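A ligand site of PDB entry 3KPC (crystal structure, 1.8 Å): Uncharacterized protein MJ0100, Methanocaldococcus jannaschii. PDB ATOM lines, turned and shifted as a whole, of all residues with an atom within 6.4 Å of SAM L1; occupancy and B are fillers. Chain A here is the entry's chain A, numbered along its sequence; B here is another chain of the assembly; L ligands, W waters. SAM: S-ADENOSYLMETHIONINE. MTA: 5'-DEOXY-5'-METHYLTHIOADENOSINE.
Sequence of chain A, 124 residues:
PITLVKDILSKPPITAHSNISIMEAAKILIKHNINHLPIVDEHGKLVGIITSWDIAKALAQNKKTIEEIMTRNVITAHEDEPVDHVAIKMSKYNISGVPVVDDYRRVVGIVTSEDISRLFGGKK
Ile 49 touches SAM L1. CG2 of Thr 51 touches C8 of SAM L1, at 3.6 Å. CE3 of Trp 53 touches C3' of SAM L1 (3.6 Å). Asn 73 touches SAM L1. Val 74 touches SAM L1 (CA to N1, 3.6 Å). Ile 95 touches SAM L1. CA of Val 98 touches N6 of SAM L1, at 3.8 Å. CD of Pro 99 touches N6 of SAM L1 (3.7 Å). Asn 33 of chain B touches SAM L1 (OD1 to CG, 3.1 Å). The nearest printed residue that does not touch SAM L1 is Tyr 93 (4.2 Å).
The backbone carbonyl oxygen (O) of Ile 75 lies within hydrogen-bond range of a nitrogen (N6) of SAM L1, at 3.1 Å. OD1 of Asn 94 lies within hydrogen-bond range of N of SAM L1. A nitrogen (N6) of SAM L1 sits at hydrogen-bond distance from the backbone carbonyl oxygen of Gly 97 (2.7 Å). The side-chain amide nitrogen (ND2) of Asn 35 of chain B sits at hydrogen-bond distance from an oxygen (OXT) of SAM L1. O of SAM L1 lies within hydrogen-bond range of N of Ser 96, at 3.3 Å. O of Asn 94 is in hydrogen-bond range of N of SAM L1 (3.0 Å). An oxygen (O2') of SAM L1 sits at hydrogen-bond distance from the side-chain hydroxyl of Thr 71, at 2.7 Å. The side-chain hydroxyl of Ser 96 lies within hydrogen-bond range of an oxygen (O) of SAM L1, 3.4 Å away. The backbone NH (N) of Ile 75 sits at hydrogen-bond distance from a nitrogen (N1) of SAM L1, at 2.9 Å. O3' of SAM L1 is in hydrogen-bond range of OD1 of Asp 54. A nitrogen (N) of SAM L1 is in salt-bridge range of the side-chain carboxylate (OE1) of Glu 114 of chain B (2.9 Å).
A ring nitrogen (NE2) of His 36 sits at hydrogen-bond distance from the side-chain hydroxyl (OG) of Ser 96, at 3.0 Å. NE1 of Trp 53 sits close to O of Ile 34 of chain B, 3.2 Å away. The backbone NH (N) of Trp 53 lies close to the side-chain hydroxyl (OG1) of Thr 51 (3.3 Å). O of Thr 71 is in hydrogen-bond range of N of Ile 49, at 3.0 Å. The backbone NH of Gly 97 lies within hydrogen-bond range of a ring nitrogen (NE2) of His 36 (3.4 Å). The backbone NH (N) of Thr 51 lies within hydrogen-bond range of the side-chain carboxylate (OD2) of Asp 54 (3.0 Å).
Water W2 lies within hydrogen-bond range of an oxygen (OXT) of SAM L1 (2.6 Å), the side-chain hydroxyl of Thr 51 (3.0 Å) and the side-chain hydroxyl of Ser 96 (3.2 Å). Water W4 lies within hydrogen-bond range of N of SAM L1, O of Asn 33 of chain B and OD1 of Asn 94. Water W1 lies within hydrogen-bond range of the side-chain hydroxyl of Ser 96 (2.4 Å), a ring nitrogen (NE2) of His 36 (3.0 Å), a nitrogen (N7) of SAM L1 (3.2 Å) and the backbone NH of Gly 97 (3.4 Å).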
ATOM      1  N   HIS A  36     -16.538  -3.120  -6.404  1.00  0.00           N
ATOM      2  CA  HIS A  36     -17.211  -3.153  -7.702  1.00  0.00           C
ATOM      3  C   HIS A  36     -16.811  -4.353  -8.542  1.00  0.00           C
ATOM      4  O   HIS A  36     -15.625  -4.664  -8.669  1.00  0.00           O
ATOM      5  CB  HIS A  36     -16.935  -1.881  -8.502  1.00  0.00           C
ATOM      6  CG  HIS A  36     -17.347  -0.639  -7.794  1.00  0.00           C
ATOM      7  ND1 HIS A  36     -16.559  -0.037  -6.837  1.00  0.00           N
ATOM      8  CD2 HIS A  36     -18.483   0.090  -7.856  1.00  0.00           C
ATOM      9  CE1 HIS A  36     -17.176   1.027  -6.358  1.00  0.00           C
ATOM     10  NE2 HIS A  36     -18.353   1.127  -6.963  1.00  0.00           N
ATOM     11  N   ILE A  49     -23.643  -4.926 -13.334  1.00  0.00           N
ATOM     12  CA  ILE A  49     -22.661  -4.635 -12.295  1.00  0.00           C
ATOM     13  C   ILE A  49     -23.170  -5.074 -10.916  1.00  0.00           C
ATOM     14  O   ILE A  49     -24.358  -4.950 -10.593  1.00  0.00           O
ATOM     15  CB  ILE A  49     -22.219  -3.138 -12.288  1.00  0.00           C
ATOM     16  CG1 ILE A  49     -20.950  -2.919 -11.459  1.00  0.00           C
ATOM     17  CG2 ILE A  49     -23.366  -2.210 -11.869  1.00  0.00           C
ATOM     18  CD1 ILE A  49     -20.290  -1.550 -11.616  1.00  0.00           C
ATOM     19  N   ILE A  50     -22.246  -5.629 -10.125  1.00  0.00           N
ATOM     20  CA  ILE A  50     -22.482  -6.020  -8.750  1.00  0.00           C
ATOM     21  C   ILE A  50     -21.580  -5.171  -7.860  1.00  0.00           C
ATOM     22  O   ILE A  50     -20.395  -4.991  -8.168  1.00  0.00           O
ATOM     23  CB  ILE A  50     -22.123  -7.521  -8.544  1.00  0.00           C
ATOM     24  CG1 ILE A  50     -23.182  -8.424  -9.183  1.00  0.00           C
ATOM     25  CG2 ILE A  50     -21.880  -7.863  -7.061  1.00  0.00           C
ATOM     26  CD1 ILE A  50     -24.507  -8.480  -8.448  1.00  0.00           C
ATOM     27  N   THR A  51     -22.132  -4.624  -6.779  1.00  0.00           N
ATOM     28  CA  THR A  51     -21.306  -3.939  -5.797  1.00  0.00           C
ATOM     29  C   THR A  51     -21.507  -4.576  -4.427  1.00  0.00           C
ATOM     30  O   THR A  51     -22.409  -5.411  -4.264  1.00  0.00           O
ATOM     31  CB  THR A  51     -21.609  -2.415  -5.717  1.00  0.00           C
ATOM     32  OG1 THR A  51     -22.893  -2.201  -5.115  1.00  0.00           O
ATOM     33  CG2 THR A  51     -21.566  -1.769  -7.102  1.00  0.00           C
ATOM     34  N   TRP A  53     -22.805  -3.268  -1.945  1.00  0.00           N
ATOM     35  CA  TRP A  53     -24.152  -2.872  -1.534  1.00  0.00           C
ATOM     36  C   TRP A  53     -25.204  -3.889  -1.988  1.00  0.00           C
ATOM     37  O   TRP A  53     -26.155  -4.186  -1.267  1.00  0.00           O
ATOM     38  CB  TRP A  53     -24.479  -1.485  -2.079  1.00  0.00           C
ATOM     39  CG  TRP A  53     -25.680  -0.840  -1.476  1.00  0.00           C
ATOM     40  CD1 TRP A  53     -25.731  -0.087  -0.339  1.00  0.00           C
ATOM     41  CD2 TRP A  53     -27.019  -0.848  -2.005  1.00  0.00           C
ATOM     42  NE1 TRP A  53     -27.012   0.366  -0.116  1.00  0.00           N
ATOM     43  CE2 TRP A  53     -27.823  -0.086  -1.134  1.00  0.00           C
ATOM     44  CE3 TRP A  53     -27.609  -1.438  -3.141  1.00  0.00           C
ATOM     45  CZ2 TRP A  53     -29.196   0.104  -1.349  1.00  0.00           C
ATOM     46  CZ3 TRP A  53     -28.974  -1.249  -3.350  1.00  0.00           C
ATOM     47  CH2 TRP A  53     -29.754  -0.480  -2.458  1.00  0.00           C
ATOM     48  N   ASP A  54     -25.017  -4.428  -3.199  1.00  0.00           N
ATOM     49  CA  ASP A  54     -25.891  -5.486  -3.710  1.00  0.00           C
ATOM     50  C   ASP A  54     -25.758  -6.787  -2.925  1.00  0.00           C
ATOM     51  O   ASP A  54     -26.753  -7.494  -2.745  1.00  0.00           O
ATOM     52  CB  ASP A  54     -25.629  -5.762  -5.198  1.00  0.00           C
ATOM     53  CG  ASP A  54     -25.935  -4.562  -6.071  1.00  0.00           C
ATOM     54  OD1 ASP A  54     -27.009  -3.955  -5.900  1.00  0.00           O
ATOM     55  OD2 ASP A  54     -25.092  -4.239  -6.931  1.00  0.00           O
ATOM     56  N   LYS A  57     -27.688  -6.187   0.053  1.00  0.00           N
ATOM     57  CA  LYS A  57     -29.110  -6.262  -0.304  1.00  0.00           C
ATOM     58  C   LYS A  57     -29.610  -7.702  -0.388  1.00  0.00           C
ATOM     59  O   LYS A  57     -30.748  -7.998   0.012  1.00  0.00           O
ATOM     60  CB  LYS A  57     -29.389  -5.530  -1.622  1.00  0.00           C
ATOM     61  CG  LYS A  57     -30.876  -5.301  -1.947  1.00  0.00           C
ATOM     62  CD  LYS A  57     -31.033  -4.430  -3.201  1.00  0.00           C
ATOM     63  CE  LYS A  57     -32.486  -3.999  -3.419  1.00  0.00           C
ATOM     64  NZ  LYS A  57     -33.255  -4.952  -4.266  1.00  0.00           N
ATOM     65  N   ILE A  69     -29.892  -9.794  -8.689  1.00  0.00           N
ATOM     66  CA  ILE A  69     -29.470  -8.604  -7.940  1.00  0.00           C
ATOM     67  C   ILE A  69     -28.604  -7.607  -8.703  1.00  0.00           C
ATOM     68  O   ILE A  69     -28.470  -6.459  -8.267  1.00  0.00           O
ATOM     69  CB  ILE A  69     -28.787  -8.968  -6.586  1.00  0.00           C
ATOM     70  CG1 ILE A  69     -27.447  -9.699  -6.808  1.00  0.00           C
ATOM     71  CG2 ILE A  69     -29.720  -9.786  -5.721  1.00  0.00           C
ATOM     72  CD1 ILE A  69     -26.570  -9.784  -5.558  1.00  0.00           C
ATOM     73  N   MET A  70     -28.009  -8.025  -9.822  1.00  0.00           N
ATOM     74  CA  MET A  70     -27.150  -7.097 -10.562  1.00  0.00           C
ATOM     75  C   MET A  70     -27.943  -5.959 -11.208  1.00  0.00           C
ATOM     76  O   MET A  70     -29.093  -6.133 -11.601  1.00  0.00           O
ATOM     77  CB  MET A  70     -26.304  -7.835 -11.614  1.00  0.00           C
ATOM     78  CG  MET A  70     -27.065  -8.392 -12.813  1.00  0.00           C
ATOM     79  SD  MET A  70     -25.929  -9.253 -13.916  1.00  0.00           S
ATOM     80  CE  MET A  70     -27.008  -9.534 -15.334  1.00  0.00           C
ATOM     81  N   THR A  71     -27.320  -4.787 -11.284  1.00  0.00           N
ATOM     82  CA  THR A  71     -27.917  -3.652 -11.986  1.00  0.00           C
ATOM     83  C   THR A  71     -27.573  -3.787 -13.458  1.00  0.00           C
ATOM     84  O   THR A  71     -26.406  -3.859 -13.822  1.00  0.00           O
ATOM     85  CB  THR A  71     -27.389  -2.310 -11.433  1.00  0.00           C
ATOM     86  OG1 THR A  71     -27.665  -2.238 -10.027  1.00  0.00           O
ATOM     87  CG2 THR A  71     -28.052  -1.133 -12.132  1.00  0.00           C
ATOM     88  N   ASN A  73     -28.830  -1.688 -16.232  1.00  0.00           N
ATOM     89  CA  ASN A  73     -28.540  -0.402 -16.903  1.00  0.00           C
ATOM     90  C   ASN A  73     -27.281   0.207 -16.292  1.00  0.00           C
ATOM     91  O   ASN A  73     -27.359   0.990 -15.341  1.00  0.00           O
ATOM     92  CB  ASN A  73     -29.737   0.565 -16.777  1.00  0.00           C
ATOM     93  CG  ASN A  73     -29.424   1.983 -17.294  1.00  0.00           C
ATOM     94  OD1 ASN A  73     -29.820   2.971 -16.675  1.00  0.00           O
ATOM     95  ND2 ASN A  73     -28.715   2.074 -18.414  1.00  0.00           N
ATOM     96  N   VAL A  74     -26.109  -0.159 -16.816  1.00  0.00           N
ATOM     97  CA  VAL A  74     -24.846   0.292 -16.226  1.00  0.00           C
ATOM     98  C   VAL A  74     -24.383   1.619 -16.813  1.00  0.00           C
ATOM     99  O   VAL A  74     -24.241   1.757 -18.042  1.00  0.00           O
ATOM    100  CB  VAL A  74     -23.720  -0.763 -16.366  1.00  0.00           C
ATOM    101  CG1 VAL A  74     -22.505  -0.381 -15.532  1.00  0.00           C
ATOM    102  CG2 VAL A  74     -24.217  -2.142 -15.947  1.00  0.00           C
ATOM    103  N   ILE A  75     -24.162   2.607 -15.943  1.00  0.00           N
ATOM    104  CA  ILE A  75     -23.533   3.870 -16.325  1.00  0.00           C
ATOM    105  C   ILE A  75     -22.029   3.611 -16.523  1.00  0.00           C
ATOM    106  O   ILE A  75     -21.371   3.055 -15.648  1.00  0.00           O
ATOM    107  CB  ILE A  75     -23.755   4.969 -15.239  1.00  0.00           C
ATOM    108  CG1 ILE A  75     -25.250   5.107 -14.876  1.00  0.00           C
ATOM    109  CG2 ILE A  75     -23.147   6.317 -15.668  1.00  0.00           C
ATOM    110  CD1 ILE A  75     -26.178   5.532 -16.030  1.00  0.00           C
ATOM    111  N   THR A  76     -21.502   4.009 -17.690  1.00  0.00           N
ATOM    112  CA  THR A  76     -20.117   3.716 -18.050  1.00  0.00           C
ATOM    113  C   THR A  76     -19.313   4.966 -18.404  1.00  0.00           C
ATOM    114  O   THR A  76     -19.879   6.053 -18.550  1.00  0.00           O
ATOM    115  CB  THR A  76     -20.031   2.735 -19.241  1.00  0.00           C
ATOM    116  OG1 THR A  76     -20.693   3.299 -20.378  1.00  0.00           O
ATOM    117  CG2 THR A  76     -20.674   1.397 -18.900  1.00  0.00           C
ATOM    118  N   TYR A  93     -26.383  10.109 -10.786  1.00  0.00           N
ATOM    119  CA  TYR A  93     -27.040   8.800 -10.650  1.00  0.00           C
ATOM    120  C   TYR A  93     -26.898   8.158  -9.280  1.00  0.00           C
ATOM    121  O   TYR A  93     -27.361   7.029  -9.063  1.00  0.00           O
ATOM    122  CB  TYR A  93     -26.604   7.848 -11.766  1.00  0.00           C
ATOM    123  CG  TYR A  93     -27.025   8.374 -13.107  1.00  0.00           C
ATOM    124  CD1 TYR A  93     -28.367   8.370 -13.487  1.00  0.00           C
ATOM    125  CD2 TYR A  93     -26.094   8.925 -13.987  1.00  0.00           C
ATOM    126  CE1 TYR A  93     -28.781   8.871 -14.720  1.00  0.00           C
ATOM    127  CE2 TYR A  93     -26.491   9.428 -15.225  1.00  0.00           C
ATOM    128  CZ  TYR A  93     -27.837   9.410 -15.585  1.00  0.00           C
ATOM    129  OH  TYR A  93     -28.235   9.907 -16.807  1.00  0.00           O
ATOM    130  N   ASN A  94     -26.280   8.895  -8.354  1.00  0.00           N
ATOM    131  CA  ASN A  94     -26.037   8.436  -6.983  1.00  0.00           C
ATOM    132  C   ASN A  94     -25.335   7.069  -6.947  1.00  0.00           C
ATOM    133  O   ASN A  94     -25.733   6.163  -6.209  1.00  0.00           O
ATOM    134  CB  ASN A  94     -27.352   8.422  -6.177  1.00  0.00           C
ATOM    135  CG  ASN A  94     -27.122   8.285  -4.680  1.00  0.00           C
ATOM    136  OD1 ASN A  94     -26.146   8.805  -4.135  1.00  0.00           O
ATOM    137  ND2 ASN A  94     -28.026   7.576  -4.002  1.00  0.00           N
ATOM    138  N   ILE A  95     -24.283   6.929  -7.744  1.00  0.00           N
ATOM    139  CA  ILE A  95     -23.517   5.681  -7.817  1.00  0.00           C
ATOM    140  C   ILE A  95     -22.075   5.934  -7.411  1.00  0.00           C
ATOM    141  O   ILE A  95     -21.642   7.085  -7.324  1.00  0.00           O
ATOM    142  CB  ILE A  95     -23.578   5.040  -9.221  1.00  0.00           C
ATOM    143  CG1 ILE A  95     -23.174   6.062 -10.291  1.00  0.00           C
ATOM    144  CG2 ILE A  95     -24.974   4.466  -9.493  1.00  0.00           C
ATOM    145  CD1 ILE A  95     -22.878   5.460 -11.648  1.00  0.00           C
ATOM    146  N   SER A  96     -21.318   4.858  -7.179  1.00  0.00           N
ATOM    147  CA  SER A  96     -19.970   5.024  -6.647  1.00  0.00           C
ATOM    148  C   SER A  96     -18.814   4.528  -7.515  1.00  0.00           C
ATOM    149  O   SER A  96     -17.646   4.659  -7.126  1.00  0.00           O
ATOM    150  CB  SER A  96     -19.871   4.439  -5.232  1.00  0.00           C
ATOM    151  OG  SER A  96     -20.013   3.030  -5.253  1.00  0.00           O
ATOM    152  N   GLY A  97     -19.118   3.972  -8.679  1.00  0.00           N
ATOM    153  CA  GLY A  97     -18.083   3.473  -9.586  1.00  0.00           C
ATOM    154  C   GLY A  97     -18.655   3.308 -10.970  1.00  0.00           C
ATOM    155  O   GLY A  97     -19.847   3.059 -11.126  1.00  0.00           O
ATOM    156  N   VAL A  98     -17.801   3.458 -11.993  1.00  0.00           N
ATOM    157  CA  VAL A  98     -18.250   3.296 -13.376  1.00  0.00           C
ATOM    158  C   VAL A  98     -17.251   2.443 -14.149  1.00  0.00           C
ATOM    159  O   VAL A  98     -16.057   2.759 -14.172  1.00  0.00           O
ATOM    160  CB  VAL A  98     -18.455   4.657 -14.107  1.00  0.00           C
ATOM    161  CG1 VAL A  98     -19.587   5.476 -13.476  1.00  0.00           C
ATOM    162  CG2 VAL A  98     -17.155   5.476 -14.157  1.00  0.00           C
ATOM    163  N   PRO A  99     -17.726   1.360 -14.785  1.00  0.00           N
ATOM    164  CA  PRO A  99     -16.809   0.624 -15.633  1.00  0.00           C
ATOM    165  C   PRO A  99     -16.394   1.461 -16.834  1.00  0.00           C
ATOM    166  O   PRO A  99     -17.201   2.219 -17.370  1.00  0.00           O
ATOM    167  CB  PRO A  99     -17.639  -0.587 -16.096  1.00  0.00           C
ATOM    168  CG  PRO A  99     -18.710  -0.726 -15.058  1.00  0.00           C
ATOM    169  CD  PRO A  99     -19.031   0.681 -14.664  1.00  0.00           C
ATOM    170  N   ASN B  33     -29.867   3.774   1.896  1.00  0.00           N
ATOM    171  CA  ASN B  33     -29.133   3.928   0.651  1.00  0.00           C
ATOM    172  C   ASN B  33     -27.702   4.394   0.890  1.00  0.00           C
ATOM    173  O   ASN B  33     -27.212   5.336   0.246  1.00  0.00           O
ATOM    174  CB  ASN B  33     -29.877   4.885  -0.272  1.00  0.00           C
ATOM    175  CG  ASN B  33     -30.149   4.286  -1.625  1.00  0.00           C
ATOM    176  OD1 ASN B  33     -29.825   4.881  -2.646  1.00  0.00           O
ATOM    177  ND2 ASN B  33     -30.758   3.112  -1.642  1.00  0.00           N
ATOM    178  N   ILE B  34     -27.039   3.731   1.830  1.00  0.00           N
ATOM    179  CA  ILE B  34     -25.698   4.088   2.273  1.00  0.00           C
ATOM    180  C   ILE B  34     -24.820   2.848   2.309  1.00  0.00           C
ATOM    181  O   ILE B  34     -25.311   1.719   2.279  1.00  0.00           O
ATOM    182  CB  ILE B  34     -25.731   4.749   3.678  1.00  0.00           C
ATOM    183  CG1 ILE B  34     -26.431   3.829   4.692  1.00  0.00           C
ATOM    184  CG2 ILE B  34     -26.420   6.122   3.607  1.00  0.00           C
ATOM    185  CD1 ILE B  34     -26.354   4.295   6.142  1.00  0.00           C
ATOM    186  N   ASN B  35     -23.511   3.066   2.392  1.00  0.00           N
ATOM    187  CA  ASN B  35     -22.548   1.969   2.495  1.00  0.00           C
ATOM    188  C   ASN B  35     -21.763   1.993   3.809  1.00  0.00           C
ATOM    189  O   ASN B  35     -20.925   1.128   4.027  1.00  0.00           O
ATOM    190  CB  ASN B  35     -21.563   2.022   1.319  1.00  0.00           C
ATOM    191  CG  ASN B  35     -22.217   1.654   0.006  1.00  0.00           C
ATOM    192  OD1 ASN B  35     -22.450   0.476  -0.274  1.00  0.00           O
ATOM    193  ND2 ASN B  35     -22.506   2.659  -0.810  1.00  0.00           N
ATOM    194  N   GLU B 114     -17.835   9.396  -2.069  1.00  0.00           N
ATOM    195  CA  GLU B 114     -18.876   9.934  -2.965  1.00  0.00           C
ATOM    196  C   GLU B 114     -19.111  11.429  -2.742  1.00  0.00           C
ATOM    197  O   GLU B 114     -19.363  12.165  -3.701  1.00  0.00           O
ATOM    198  CB  GLU B 114     -20.183   9.161  -2.818  1.00  0.00           C
ATOM    199  CG  GLU B 114     -20.109   7.717  -3.313  1.00  0.00           C
ATOM    200  CD  GLU B 114     -21.405   6.966  -3.121  1.00  0.00           C
ATOM    201  OE1 GLU B 114     -22.469   7.484  -3.520  1.00  0.00           O
ATOM    202  OE2 GLU B 114     -21.366   5.848  -2.570  1.00  0.00           O
HETATM  203  N   SAM L   1     -24.780   5.819  -3.348  1.00  0.00           N
HETATM  204  CA  SAM L   1     -24.771   4.418  -2.830  1.00  0.00           C
HETATM  205  C   SAM L   1     -23.887   3.516  -3.703  1.00  0.00           C
HETATM  206  O   SAM L   1     -23.263   3.971  -4.669  1.00  0.00           O
HETATM  207  OXT SAM L   1     -23.764   2.315  -3.467  1.00  0.00           O
HETATM  208  CB  SAM L   1     -26.205   3.850  -2.755  1.00  0.00           C
HETATM  209  CG  SAM L   1     -27.069   4.203  -3.972  1.00  0.00           C
HETATM  210  SD  SAM L   1     -26.599   3.306  -5.499  1.00  0.00           S
HETATM  211  CE  SAM L   1     -27.999   3.736  -6.519  1.00  0.00           C
HETATM  212  C5' SAM L   1     -26.863   1.502  -5.256  1.00  0.00           C
HETATM  213  C4' SAM L   1     -26.877   0.738  -6.589  1.00  0.00           C
HETATM  214  O4' SAM L   1     -25.903   1.367  -7.451  1.00  0.00           O
HETATM  215  C3' SAM L   1     -26.432  -0.725  -6.497  1.00  0.00           C
HETATM  216  O3' SAM L   1     -27.555  -1.558  -6.803  1.00  0.00           O
HETATM  217  C2' SAM L   1     -25.371  -0.852  -7.592  1.00  0.00           C
HETATM  218  O2' SAM L   1     -25.535  -2.044  -8.376  1.00  0.00           O
HETATM  219  C1' SAM L   1     -25.661   0.384  -8.439  1.00  0.00           C
HETATM  220  N9  SAM L   1     -24.502   0.794  -9.264  1.00  0.00           N
HETATM  221  C8  SAM L   1     -23.232   0.890  -8.875  1.00  0.00           C
HETATM  222  N7  SAM L   1     -22.474   1.278  -9.897  1.00  0.00           N
HETATM  223  C5  SAM L   1     -23.271   1.436 -10.952  1.00  0.00           C
HETATM  224  C6  SAM L   1     -23.072   1.815 -12.276  1.00  0.00           C
HETATM  225  N6  SAM L   1     -21.855   2.127 -12.731  1.00  0.00           N
HETATM  226  N1  SAM L   1     -24.130   1.868 -13.107  1.00  0.00           N
HETATM  227  C2  SAM L   1     -25.359   1.562 -12.687  1.00  0.00           C
HETATM  228  N3  SAM L   1     -25.569   1.200 -11.430  1.00  0.00           N
HETATM  229  C4  SAM L   1     -24.552   1.126 -10.546  1.00  0.00           C
HETATM  230  CS  MTA L   2     -22.171   5.593   2.161  1.00  0.00           C
HETATM  231  S5' MTA L   2     -22.188   6.438   0.602  1.00  0.00           S
HETATM  232  C5' MTA L   2     -23.908   7.121   0.680  1.00  0.00           C
HETATM  233  C4' MTA L   2     -23.997   8.683   0.856  1.00  0.00           C
HETATM  234  O4' MTA L   2     -24.948   8.991   1.920  1.00  0.00           O
HETATM  235  C2' MTA L   2     -22.797   9.772   2.668  1.00  0.00           C
HETATM  236  O2' MTA L   2     -22.449  11.215   2.833  1.00  0.00           O
HETATM  237  C3' MTA L   2     -22.649   9.301   1.230  1.00  0.00           C
HETATM  238  O3' MTA L   2     -22.323  10.425   0.327  1.00  0.00           O
HETATM  239  C1' MTA L   2     -24.234   9.480   3.093  1.00  0.00           C
HETATM  240  N9  MTA L   2     -24.023   8.509   4.217  1.00  0.00           N
HETATM  241  C8  MTA L   2     -23.227   7.447   4.232  1.00  0.00           C
HETATM  242  N7  MTA L   2     -23.283   6.831   5.413  1.00  0.00           N
HETATM  243  C5  MTA L   2     -24.124   7.527   6.173  1.00  0.00           C
HETATM  244  C6  MTA L   2     -24.585   7.384   7.472  1.00  0.00           C
HETATM  245  N6  MTA L   2     -24.165   6.384   8.242  1.00  0.00           N
HETATM  246  N1  MTA L   2     -25.455   8.298   7.950  1.00  0.00           N
HETATM  247  C2  MTA L   2     -25.888   9.297   7.198  1.00  0.00           C
HETATM  248  N3  MTA L   2     -25.461   9.463   5.957  1.00  0.00           N
HETATM  249  C4  MTA L   2     -24.587   8.596   5.416  1.00  0.00           C
HETATM  250  O   HOH W   1     -21.250   1.923  -7.036  1.00  0.00           O
HETATM  251  O   HOH W   2     -22.231   0.718  -4.835  1.00  0.00           O
HETATM  252  O   HOH W   3     -30.197  -0.837  -6.858  1.00  0.00           O
HETATM  253  O   HOH W   4     -26.063   7.309  -1.371  1.00  0.00           O
HETATM  254  O   HOH W   5     -30.819   5.098  -7.963  1.00  0.00           O
HETATM  255  O   HOH W   6     -28.123   2.267 -10.038  1.00  0.00           O
HETATM  256  O   HOH W   7     -30.142   2.477  -4.364  1.00  0.00           O
